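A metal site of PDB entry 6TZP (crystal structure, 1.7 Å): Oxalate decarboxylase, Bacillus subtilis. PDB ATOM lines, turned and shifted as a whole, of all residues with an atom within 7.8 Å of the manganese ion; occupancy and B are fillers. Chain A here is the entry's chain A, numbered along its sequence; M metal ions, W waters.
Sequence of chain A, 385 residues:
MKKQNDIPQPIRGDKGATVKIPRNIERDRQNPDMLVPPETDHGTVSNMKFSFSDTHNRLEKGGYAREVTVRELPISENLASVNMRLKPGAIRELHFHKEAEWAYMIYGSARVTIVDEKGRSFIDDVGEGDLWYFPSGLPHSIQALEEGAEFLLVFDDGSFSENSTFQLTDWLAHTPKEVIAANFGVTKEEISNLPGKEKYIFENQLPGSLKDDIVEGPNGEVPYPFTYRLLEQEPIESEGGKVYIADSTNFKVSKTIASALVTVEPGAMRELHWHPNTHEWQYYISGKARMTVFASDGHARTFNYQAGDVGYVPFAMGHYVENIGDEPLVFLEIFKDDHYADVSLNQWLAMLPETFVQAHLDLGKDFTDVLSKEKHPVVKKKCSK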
ATOM      1  N   VAL A 262       4.626  12.356 -24.430  1.00  0.00           N
ATOM      2  CA  VAL A 262       3.889  11.832 -25.571  1.00  0.00           C
ATOM      3  C   VAL A 262       4.775  10.848 -26.321  1.00  0.00           C
ATOM      4  O   VAL A 262       5.925  11.148 -26.641  1.00  0.00           O
ATOM      5  CB  VAL A 262       3.457  12.983 -26.505  1.00  0.00           C
ATOM      6  CG1 VAL A 262       2.567  12.416 -27.633  1.00  0.00           C
ATOM      7  CG2 VAL A 262       2.752  14.075 -25.707  1.00  0.00           C
ATOM      8  N   ARG A 270       0.619  13.089 -33.267  1.00  0.00           N
ATOM      9  CA  ARG A 270      -0.156  13.876 -32.310  1.00  0.00           C
ATOM     10  C   ARG A 270      -1.142  14.722 -33.101  1.00  0.00           C
ATOM     11  O   ARG A 270      -0.744  15.484 -33.984  1.00  0.00           O
ATOM     12  CB  ARG A 270       0.784  14.753 -31.479  1.00  0.00           C
ATOM     13  CG  ARG A 270       0.108  15.675 -30.459  1.00  0.00           C
ATOM     14  CD  ARG A 270      -0.260  14.933 -29.157  1.00  0.00           C
ATOM     15  NE  ARG A 270      -0.792  15.868 -28.171  1.00  0.00           N
ATOM     16  CZ  ARG A 270      -2.069  16.224 -28.075  1.00  0.00           C
ATOM     17  NH1 ARG A 270      -2.967  15.706 -28.916  1.00  0.00           N
ATOM     18  NH2 ARG A 270      -2.456  17.085 -27.143  1.00  0.00           N
ATOM     19  N   GLU A 271      -2.438  14.554 -32.809  1.00  0.00           N
ATOM     20  CA  GLU A 271      -3.499  15.081 -33.669  1.00  0.00           C
ATOM     21  C   GLU A 271      -3.515  16.615 -33.685  1.00  0.00           C
ATOM     22  O   GLU A 271      -2.876  17.296 -32.868  1.00  0.00           O
ATOM     23  CB  GLU A 271      -4.871  14.565 -33.216  1.00  0.00           C
ATOM     24  CG  GLU A 271      -5.304  15.127 -31.847  1.00  0.00           C
ATOM     25  CD  GLU A 271      -6.784  14.899 -31.540  1.00  0.00           C
ATOM     26  OE1 GLU A 271      -7.546  14.549 -32.457  1.00  0.00           O
ATOM     27  OE2 GLU A 271      -7.164  15.065 -30.350  1.00  0.00           O
ATOM     28  N   HIS A 273      -4.617  20.086 -32.789  1.00  0.00           N
ATOM     29  CA  HIS A 273      -5.137  20.544 -31.510  1.00  0.00           C
ATOM     30  C   HIS A 273      -4.554  21.925 -31.204  1.00  0.00           C
ATOM     31  O   HIS A 273      -3.659  22.414 -31.885  1.00  0.00           O
ATOM     32  CB  HIS A 273      -4.820  19.549 -30.373  1.00  0.00           C
ATOM     33  CG  HIS A 273      -3.376  19.524 -29.961  1.00  0.00           C
ATOM     34  ND1 HIS A 273      -2.393  18.892 -30.707  1.00  0.00           N
ATOM     35  CD2 HIS A 273      -2.752  20.037 -28.876  1.00  0.00           C
ATOM     36  CE1 HIS A 273      -1.223  19.036 -30.098  1.00  0.00           C
ATOM     37  NE2 HIS A 273      -1.414  19.721 -28.991  1.00  0.00           N
ATOM     38  N   TRP A 274      -5.091  22.545 -30.144  1.00  0.00           N
ATOM     39  CA  TRP A 274      -4.453  23.719 -29.574  1.00  0.00           C
ATOM     40  C   TRP A 274      -4.649  23.710 -28.064  1.00  0.00           C
ATOM     41  O   TRP A 274      -5.387  22.878 -27.525  1.00  0.00           O
ATOM     42  CB  TRP A 274      -4.968  25.017 -30.196  1.00  0.00           C
ATOM     43  CG  TRP A 274      -6.376  25.434 -29.784  1.00  0.00           C
ATOM     44  CD1 TRP A 274      -6.718  26.342 -28.811  1.00  0.00           C
ATOM     45  CD2 TRP A 274      -7.601  24.977 -30.366  1.00  0.00           C
ATOM     46  NE1 TRP A 274      -8.090  26.452 -28.730  1.00  0.00           N
ATOM     47  CE2 TRP A 274      -8.656  25.648 -29.688  1.00  0.00           C
ATOM     48  CE3 TRP A 274      -7.921  24.077 -31.385  1.00  0.00           C
ATOM     49  CZ2 TRP A 274     -10.007  25.433 -30.008  1.00  0.00           C
ATOM     50  CZ3 TRP A 274      -9.262  23.875 -31.700  1.00  0.00           C
ATOM     51  CH2 TRP A 274     -10.284  24.557 -31.012  1.00  0.00           C
ATOM     52  N   HIS A 275      -3.955  24.620 -27.394  1.00  0.00           N
ATOM     53  CA  HIS A 275      -4.060  24.736 -25.944  1.00  0.00           C
ATOM     54  C   HIS A 275      -4.720  26.056 -25.586  1.00  0.00           C
ATOM     55  O   HIS A 275      -4.226  27.121 -25.973  1.00  0.00           O
ATOM     56  CB  HIS A 275      -2.669  24.623 -25.306  1.00  0.00           C
ATOM     57  CG  HIS A 275      -2.000  23.333 -25.643  1.00  0.00           C
ATOM     58  ND1 HIS A 275      -2.414  22.135 -25.100  1.00  0.00           N
ATOM     59  CD2 HIS A 275      -1.033  23.026 -26.543  1.00  0.00           C
ATOM     60  CE1 HIS A 275      -1.700  21.144 -25.627  1.00  0.00           C
ATOM     61  NE2 HIS A 275      -0.862  21.666 -26.507  1.00  0.00           N
ATOM     62  N   GLU A 280       3.082  26.404 -25.236  1.00  0.00           N
ATOM     63  CA  GLU A 280       3.685  25.078 -25.114  1.00  0.00           C
ATOM     64  C   GLU A 280       5.183  25.165 -25.375  1.00  0.00           C
ATOM     65  O   GLU A 280       5.618  25.738 -26.380  1.00  0.00           O
ATOM     66  CB  GLU A 280       3.068  24.077 -26.116  1.00  0.00           C
ATOM     67  CG  GLU A 280       3.728  22.692 -26.086  1.00  0.00           C
ATOM     68  CD  GLU A 280       3.011  21.686 -26.984  1.00  0.00           C
ATOM     69  OE1 GLU A 280       1.773  21.775 -27.088  1.00  0.00           O
ATOM     70  OE2 GLU A 280       3.671  20.818 -27.579  1.00  0.00           O
ATOM     71  N   TRP A 281       5.975  24.555 -24.484  1.00  0.00           N
ATOM     72  CA  TRP A 281       7.413  24.384 -24.667  1.00  0.00           C
ATOM     73  C   TRP A 281       7.663  22.890 -24.880  1.00  0.00           C
ATOM     74  O   TRP A 281       7.006  22.064 -24.236  1.00  0.00           O
ATOM     75  CB  TRP A 281       8.154  24.895 -23.430  1.00  0.00           C
ATOM     76  CG  TRP A 281       9.635  24.871 -23.505  1.00  0.00           C
ATOM     77  CD1 TRP A 281      10.445  25.921 -23.818  1.00  0.00           C
ATOM     78  CD2 TRP A 281      10.485  23.763 -23.209  1.00  0.00           C
ATOM     79  NE1 TRP A 281      11.763  25.523 -23.758  1.00  0.00           N
ATOM     80  CE2 TRP A 281      11.810  24.203 -23.386  1.00  0.00           C
ATOM     81  CE3 TRP A 281      10.265  22.431 -22.820  1.00  0.00           C
ATOM     82  CZ2 TRP A 281      12.918  23.365 -23.201  1.00  0.00           C
ATOM     83  CZ3 TRP A 281      11.363  21.595 -22.625  1.00  0.00           C
ATOM     84  CH2 TRP A 281      12.674  22.071 -22.813  1.00  0.00           C
ATOM     85  N   GLN A 282       8.559  22.540 -25.809  1.00  0.00           N
ATOM     86  CA  GLN A 282       8.742  21.134 -26.194  1.00  0.00           C
ATOM     87  C   GLN A 282      10.184  20.698 -26.048  1.00  0.00           C
ATOM     88  O   GLN A 282      11.108  21.471 -26.322  1.00  0.00           O
ATOM     89  CB  GLN A 282       8.350  20.869 -27.667  1.00  0.00           C
ATOM     90  CG  GLN A 282       6.950  21.313 -28.060  1.00  0.00           C
ATOM     91  CD  GLN A 282       6.688  21.088 -29.538  1.00  0.00           C
ATOM     92  OE1 GLN A 282       7.607  21.152 -30.368  1.00  0.00           O
ATOM     93  NE2 GLN A 282       5.437  20.820 -29.880  1.00  0.00           N
ATOM     94  N   MET A 291       6.246  19.617 -37.434  1.00  0.00           N
ATOM     95  CA  MET A 291       5.077  20.288 -36.853  1.00  0.00           C
ATOM     96  C   MET A 291       4.825  21.564 -37.635  1.00  0.00           C
ATOM     97  O   MET A 291       5.758  22.340 -37.861  1.00  0.00           O
ATOM     98  CB  MET A 291       5.311  20.632 -35.369  1.00  0.00           C
ATOM     99  CG  MET A 291       4.348  21.696 -34.808  1.00  0.00           C
ATOM    100  SD  MET A 291       4.462  22.021 -33.011  1.00  0.00           S
ATOM    101  CE  MET A 291       6.034  22.890 -32.900  1.00  0.00           C
ATOM    102  N   VAL A 313       5.266  26.390 -29.078  1.00  0.00           N
ATOM    103  CA  VAL A 313       4.002  26.750 -29.719  1.00  0.00           C
ATOM    104  C   VAL A 313       3.367  27.877 -28.920  1.00  0.00           C
ATOM    105  O   VAL A 313       2.876  27.650 -27.808  1.00  0.00           O
ATOM    106  CB  VAL A 313       3.032  25.564 -29.811  1.00  0.00           C
ATOM    107  CG1 VAL A 313       1.782  25.944 -30.611  1.00  0.00           C
ATOM    108  CG2 VAL A 313       3.692  24.327 -30.454  1.00  0.00           C
ATOM    109  N   MET A 317      -1.962  28.714 -30.623  1.00  0.00           N
ATOM    110  CA  MET A 317      -1.704  28.430 -32.040  1.00  0.00           C
ATOM    111  C   MET A 317      -2.004  26.967 -32.356  1.00  0.00           C
ATOM    112  O   MET A 317      -1.726  26.062 -31.552  1.00  0.00           O
ATOM    113  CB  MET A 317      -0.254  28.773 -32.382  1.00  0.00           C
ATOM    114  CG  MET A 317       0.010  30.279 -32.286  1.00  0.00           C
ATOM    115  SD  MET A 317       1.535  30.723 -33.150  1.00  0.00           S
ATOM    116  CE  MET A 317       1.494  32.514 -32.981  1.00  0.00           C
ATOM    117  N   GLY A 318      -2.576  26.717 -33.539  1.00  0.00           N
ATOM    118  CA  GLY A 318      -2.944  25.358 -33.923  1.00  0.00           C
ATOM    119  C   GLY A 318      -1.720  24.578 -34.350  1.00  0.00           C
ATOM    120  O   GLY A 318      -0.792  25.115 -34.931  1.00  0.00           O
ATOM    121  N   HIS A 319      -1.710  23.280 -34.026  1.00  0.00           N
ATOM    122  CA  HIS A 319      -0.537  22.473 -34.357  1.00  0.00           C
ATOM    123  C   HIS A 319      -0.869  20.974 -34.322  1.00  0.00           C
ATOM    124  O   HIS A 319      -1.924  20.559 -33.848  1.00  0.00           O
ATOM    125  CB  HIS A 319       0.638  22.805 -33.411  1.00  0.00           C
ATOM    126  CG  HIS A 319       0.341  22.625 -31.949  1.00  0.00           C
ATOM    127  ND1 HIS A 319      -0.507  23.463 -31.260  1.00  0.00           N
ATOM    128  CD2 HIS A 319       0.832  21.743 -31.047  1.00  0.00           C
ATOM    129  CE1 HIS A 319      -0.556  23.083 -29.983  1.00  0.00           C
ATOM    130  NE2 HIS A 319       0.253  22.046 -29.829  1.00  0.00           N
ATOM    131  N   TYR A 320       0.049  20.202 -34.892  1.00  0.00           N
ATOM    132  CA  TYR A 320       0.089  18.746 -34.839  1.00  0.00           C
ATOM    133  C   TYR A 320       1.564  18.368 -34.724  1.00  0.00           C
ATOM    134  O   TYR A 320       2.438  19.189 -35.016  1.00  0.00           O
ATOM    135  CB  TYR A 320      -0.520  18.109 -36.091  1.00  0.00           C
ATOM    136  CG  TYR A 320       0.309  18.437 -37.319  1.00  0.00           C
ATOM    137  CD1 TYR A 320       0.123  19.626 -38.002  1.00  0.00           C
ATOM    138  CD2 TYR A 320       1.323  17.587 -37.732  1.00  0.00           C
ATOM    139  CE1 TYR A 320       0.899  19.928 -39.118  1.00  0.00           C
ATOM    140  CE2 TYR A 320       2.120  17.888 -38.828  1.00  0.00           C
ATOM    141  CZ  TYR A 320       1.897  19.075 -39.515  1.00  0.00           C
ATOM    142  OH  TYR A 320       2.680  19.392 -40.608  1.00  0.00           O
ATOM    143  N   VAL A 321       1.868  17.143 -34.327  1.00  0.00           N
ATOM    144  CA  VAL A 321       3.268  16.673 -34.312  1.00  0.00           C
ATOM    145  C   VAL A 321       3.301  15.298 -34.973  1.00  0.00           C
ATOM    146  O   VAL A 321       2.836  14.318 -34.379  1.00  0.00           O
ATOM    147  CB  VAL A 321       3.873  16.630 -32.905  1.00  0.00           C
ATOM    148  CG1 VAL A 321       5.397  16.398 -32.993  1.00  0.00           C
ATOM    149  CG2 VAL A 321       3.584  17.929 -32.125  1.00  0.00           C
ATOM    150  N   PHE A 331       8.380  12.876 -27.018  1.00  0.00           N
ATOM    151  CA  PHE A 331       8.641  14.267 -26.694  1.00  0.00           C
ATOM    152  C   PHE A 331       7.806  14.704 -25.490  1.00  0.00           C
ATOM    153  O   PHE A 331       6.826  14.042 -25.108  1.00  0.00           O
ATOM    154  CB  PHE A 331       8.398  15.210 -27.896  1.00  0.00           C
ATOM    155  CG  PHE A 331       6.956  15.280 -28.366  1.00  0.00           C
ATOM    156  CD1 PHE A 331       6.442  14.333 -29.242  1.00  0.00           C
ATOM    157  CD2 PHE A 331       6.130  16.325 -27.966  1.00  0.00           C
ATOM    158  CE1 PHE A 331       5.116  14.397 -29.690  1.00  0.00           C
ATOM    159  CE2 PHE A 331       4.802  16.411 -28.410  1.00  0.00           C
ATOM    160  CZ  PHE A 331       4.301  15.449 -29.271  1.00  0.00           C
ATOM    161  N   GLU A 333       5.582  17.879 -23.697  1.00  0.00           N
ATOM    162  CA  GLU A 333       4.839  19.133 -23.806  1.00  0.00           C
ATOM    163  C   GLU A 333       4.815  19.783 -22.426  1.00  0.00           C
ATOM    164  O   GLU A 333       4.348  19.167 -21.462  1.00  0.00           O
ATOM    165  CB  GLU A 333       3.390  18.889 -24.272  1.00  0.00           C
ATOM    166  CG  GLU A 333       3.226  18.054 -25.523  1.00  0.00           C
ATOM    167  CD  GLU A 333       1.780  17.598 -25.713  1.00  0.00           C
ATOM    168  OE1 GLU A 333       1.083  17.420 -24.688  1.00  0.00           O
ATOM    169  OE2 GLU A 333       1.354  17.416 -26.872  1.00  0.00           O
ATOM    170  N   ILE A 334       5.324  21.019 -22.326  1.00  0.00           N
ATOM    171  CA  ILE A 334       5.488  21.699 -21.041  1.00  0.00           C
ATOM    172  C   ILE A 334       4.730  23.026 -21.073  1.00  0.00           C
ATOM    173  O   ILE A 334       4.775  23.755 -22.066  1.00  0.00           O
ATOM    174  CB  ILE A 334       6.981  21.945 -20.722  1.00  0.00           C
ATOM    175  CG1 ILE A 334       7.783  20.631 -20.721  1.00  0.00           C
ATOM    176  CG2 ILE A 334       7.131  22.647 -19.376  1.00  0.00           C
ATOM    177  CD1 ILE A 334       7.353  19.657 -19.613  1.00  0.00           C
ATOM    178  N   PHE A 335       4.028  23.335 -19.972  1.00  0.00           N
ATOM    179  CA  PHE A 335       3.195  24.539 -19.889  1.00  0.00           C
ATOM    180  C   PHE A 335       3.409  25.239 -18.552  1.00  0.00           C
ATOM    181  O   PHE A 335       3.468  24.579 -17.505  1.00  0.00           O
ATOM    182  CB  PHE A 335       1.698  24.195 -20.034  1.00  0.00           C
ATOM    183  CG  PHE A 335       1.395  23.369 -21.240  1.00  0.00           C
ATOM    184  CD1 PHE A 335       1.557  21.995 -21.210  1.00  0.00           C
ATOM    185  CD2 PHE A 335       1.018  23.973 -22.436  1.00  0.00           C
ATOM    186  CE1 PHE A 335       1.312  21.218 -22.343  1.00  0.00           C
ATOM    187  CE2 PHE A 335       0.775  23.209 -23.571  1.00  0.00           C
ATOM    188  CZ  PHE A 335       0.918  21.840 -23.520  1.00  0.00           C
ATOM    189  N   TYR A 340      -2.981  21.000 -17.289  1.00  0.00           N
ATOM    190  CA  TYR A 340      -2.913  20.691 -18.711  1.00  0.00           C
ATOM    191  C   TYR A 340      -4.299  20.841 -19.323  1.00  0.00           C
ATOM    192  O   TYR A 340      -5.294  20.391 -18.754  1.00  0.00           O
ATOM    193  CB  TYR A 340      -2.406  19.263 -18.914  1.00  0.00           C
ATOM    194  CG  TYR A 340      -2.252  18.847 -20.360  1.00  0.00           C
ATOM    195  CD1 TYR A 340      -3.346  18.387 -21.094  1.00  0.00           C
ATOM    196  CD2 TYR A 340      -1.013  18.914 -20.988  1.00  0.00           C
ATOM    197  CE1 TYR A 340      -3.203  18.006 -22.410  1.00  0.00           C
ATOM    198  CE2 TYR A 340      -0.864  18.539 -22.311  1.00  0.00           C
ATOM    199  CZ  TYR A 340      -1.959  18.074 -23.015  1.00  0.00           C
ATOM    200  OH  TYR A 340      -1.803  17.699 -24.330  1.00  0.00           O
ATOM    201  N   ALA A 341      -4.370  21.447 -20.506  1.00  0.00           N
ATOM    202  CA  ALA A 341      -5.631  21.541 -21.223  1.00  0.00           C
ATOM    203  C   ALA A 341      -5.361  21.556 -22.723  1.00  0.00           C
ATOM    204  O   ALA A 341      -4.437  22.235 -23.162  1.00  0.00           O
ATOM    205  CB  ALA A 341      -6.407  22.821 -20.848  1.00  0.00           C
ATOM    206  N   ASP A 342      -6.165  20.817 -23.487  1.00  0.00           N
ATOM    207  CA  ASP A 342      -6.132  20.926 -24.936  1.00  0.00           C
ATOM    208  C   ASP A 342      -7.548  20.863 -25.499  1.00  0.00           C
ATOM    209  O   ASP A 342      -8.477  20.383 -24.842  1.00  0.00           O
ATOM    210  CB  ASP A 342      -5.217  19.874 -25.604  1.00  0.00           C
ATOM    211  CG  ASP A 342      -5.696  18.421 -25.442  1.00  0.00           C
ATOM    212  OD1 ASP A 342      -6.552  18.127 -24.590  1.00  0.00           O
ATOM    213  OD2 ASP A 342      -5.150  17.557 -26.164  1.00  0.00           O
HETATM  214 MN    MN M   1       0.333  20.725 -28.057  1.00  0.00          MN
HETATM  215  O   HOH W   1       1.799  19.261 -28.716  1.00  0.00           O
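OE2 of Glu 280 lies within hydrogen-bond range of NE2 of Gln 282 (2.9 Å). The backbone carbonyl oxygen (O) of Glu 280 is in hydrogen-bond range of the backbone NH (N) of Val 313 (2.8 Å). The backbone carbonyl oxygen of Ala 341 is in hydrogen-bond range of a ring nitrogen (ND1) of His 275, at 2.8 Å. ND1 of His 319 lies within hydrogen-bond range of O of Met 317, at 2.9 Å. The guanidinium group (NH2) of Arg 270 lies close to a ring nitrogen (NE2) of His 273, 3.4 Å away. The backbone carbonyl oxygen (O) of Glu 271 is in hydrogen-bond range of a ring nitrogen (ND1) of His 273. The side-chain carboxylate (OE2) of Glu 333 lies within salt-bridge range of the guanidinium group (NE) of Arg 270. OE1 of Glu 333 is in hydrogen-bond range of OH of Tyr 340 (2.9 Å).
OE2 of Glu 333 touches the manganese ion (3.7 Å). Within 4 Å of the manganese ion: His 273, His 275, Glu 280, His 319 and Glu 333. The nearest printed residue that does not touch the manganese ion is Arg 270 (4.7 Å).
Water W1 bridges the side-chain carboxylate (OE2) of Glu 333 (2.6 Å) and the side-chain carboxylate (OE2) of Glu 280 (2.7 Å).
The manganese ion is bound by the side-chain carboxylate (OE1) of Glu 280 (2.0 Å), a ring nitrogen (NE2) of His 275 (2.2 Å), water W1 (2.2 Å), a ring nitrogen (NE2) of His 319 (2.2 Å) and a ring nitrogen (NE2) of His 273 (2.2 Å). The manganese ion has five donor atoms within binding distance.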
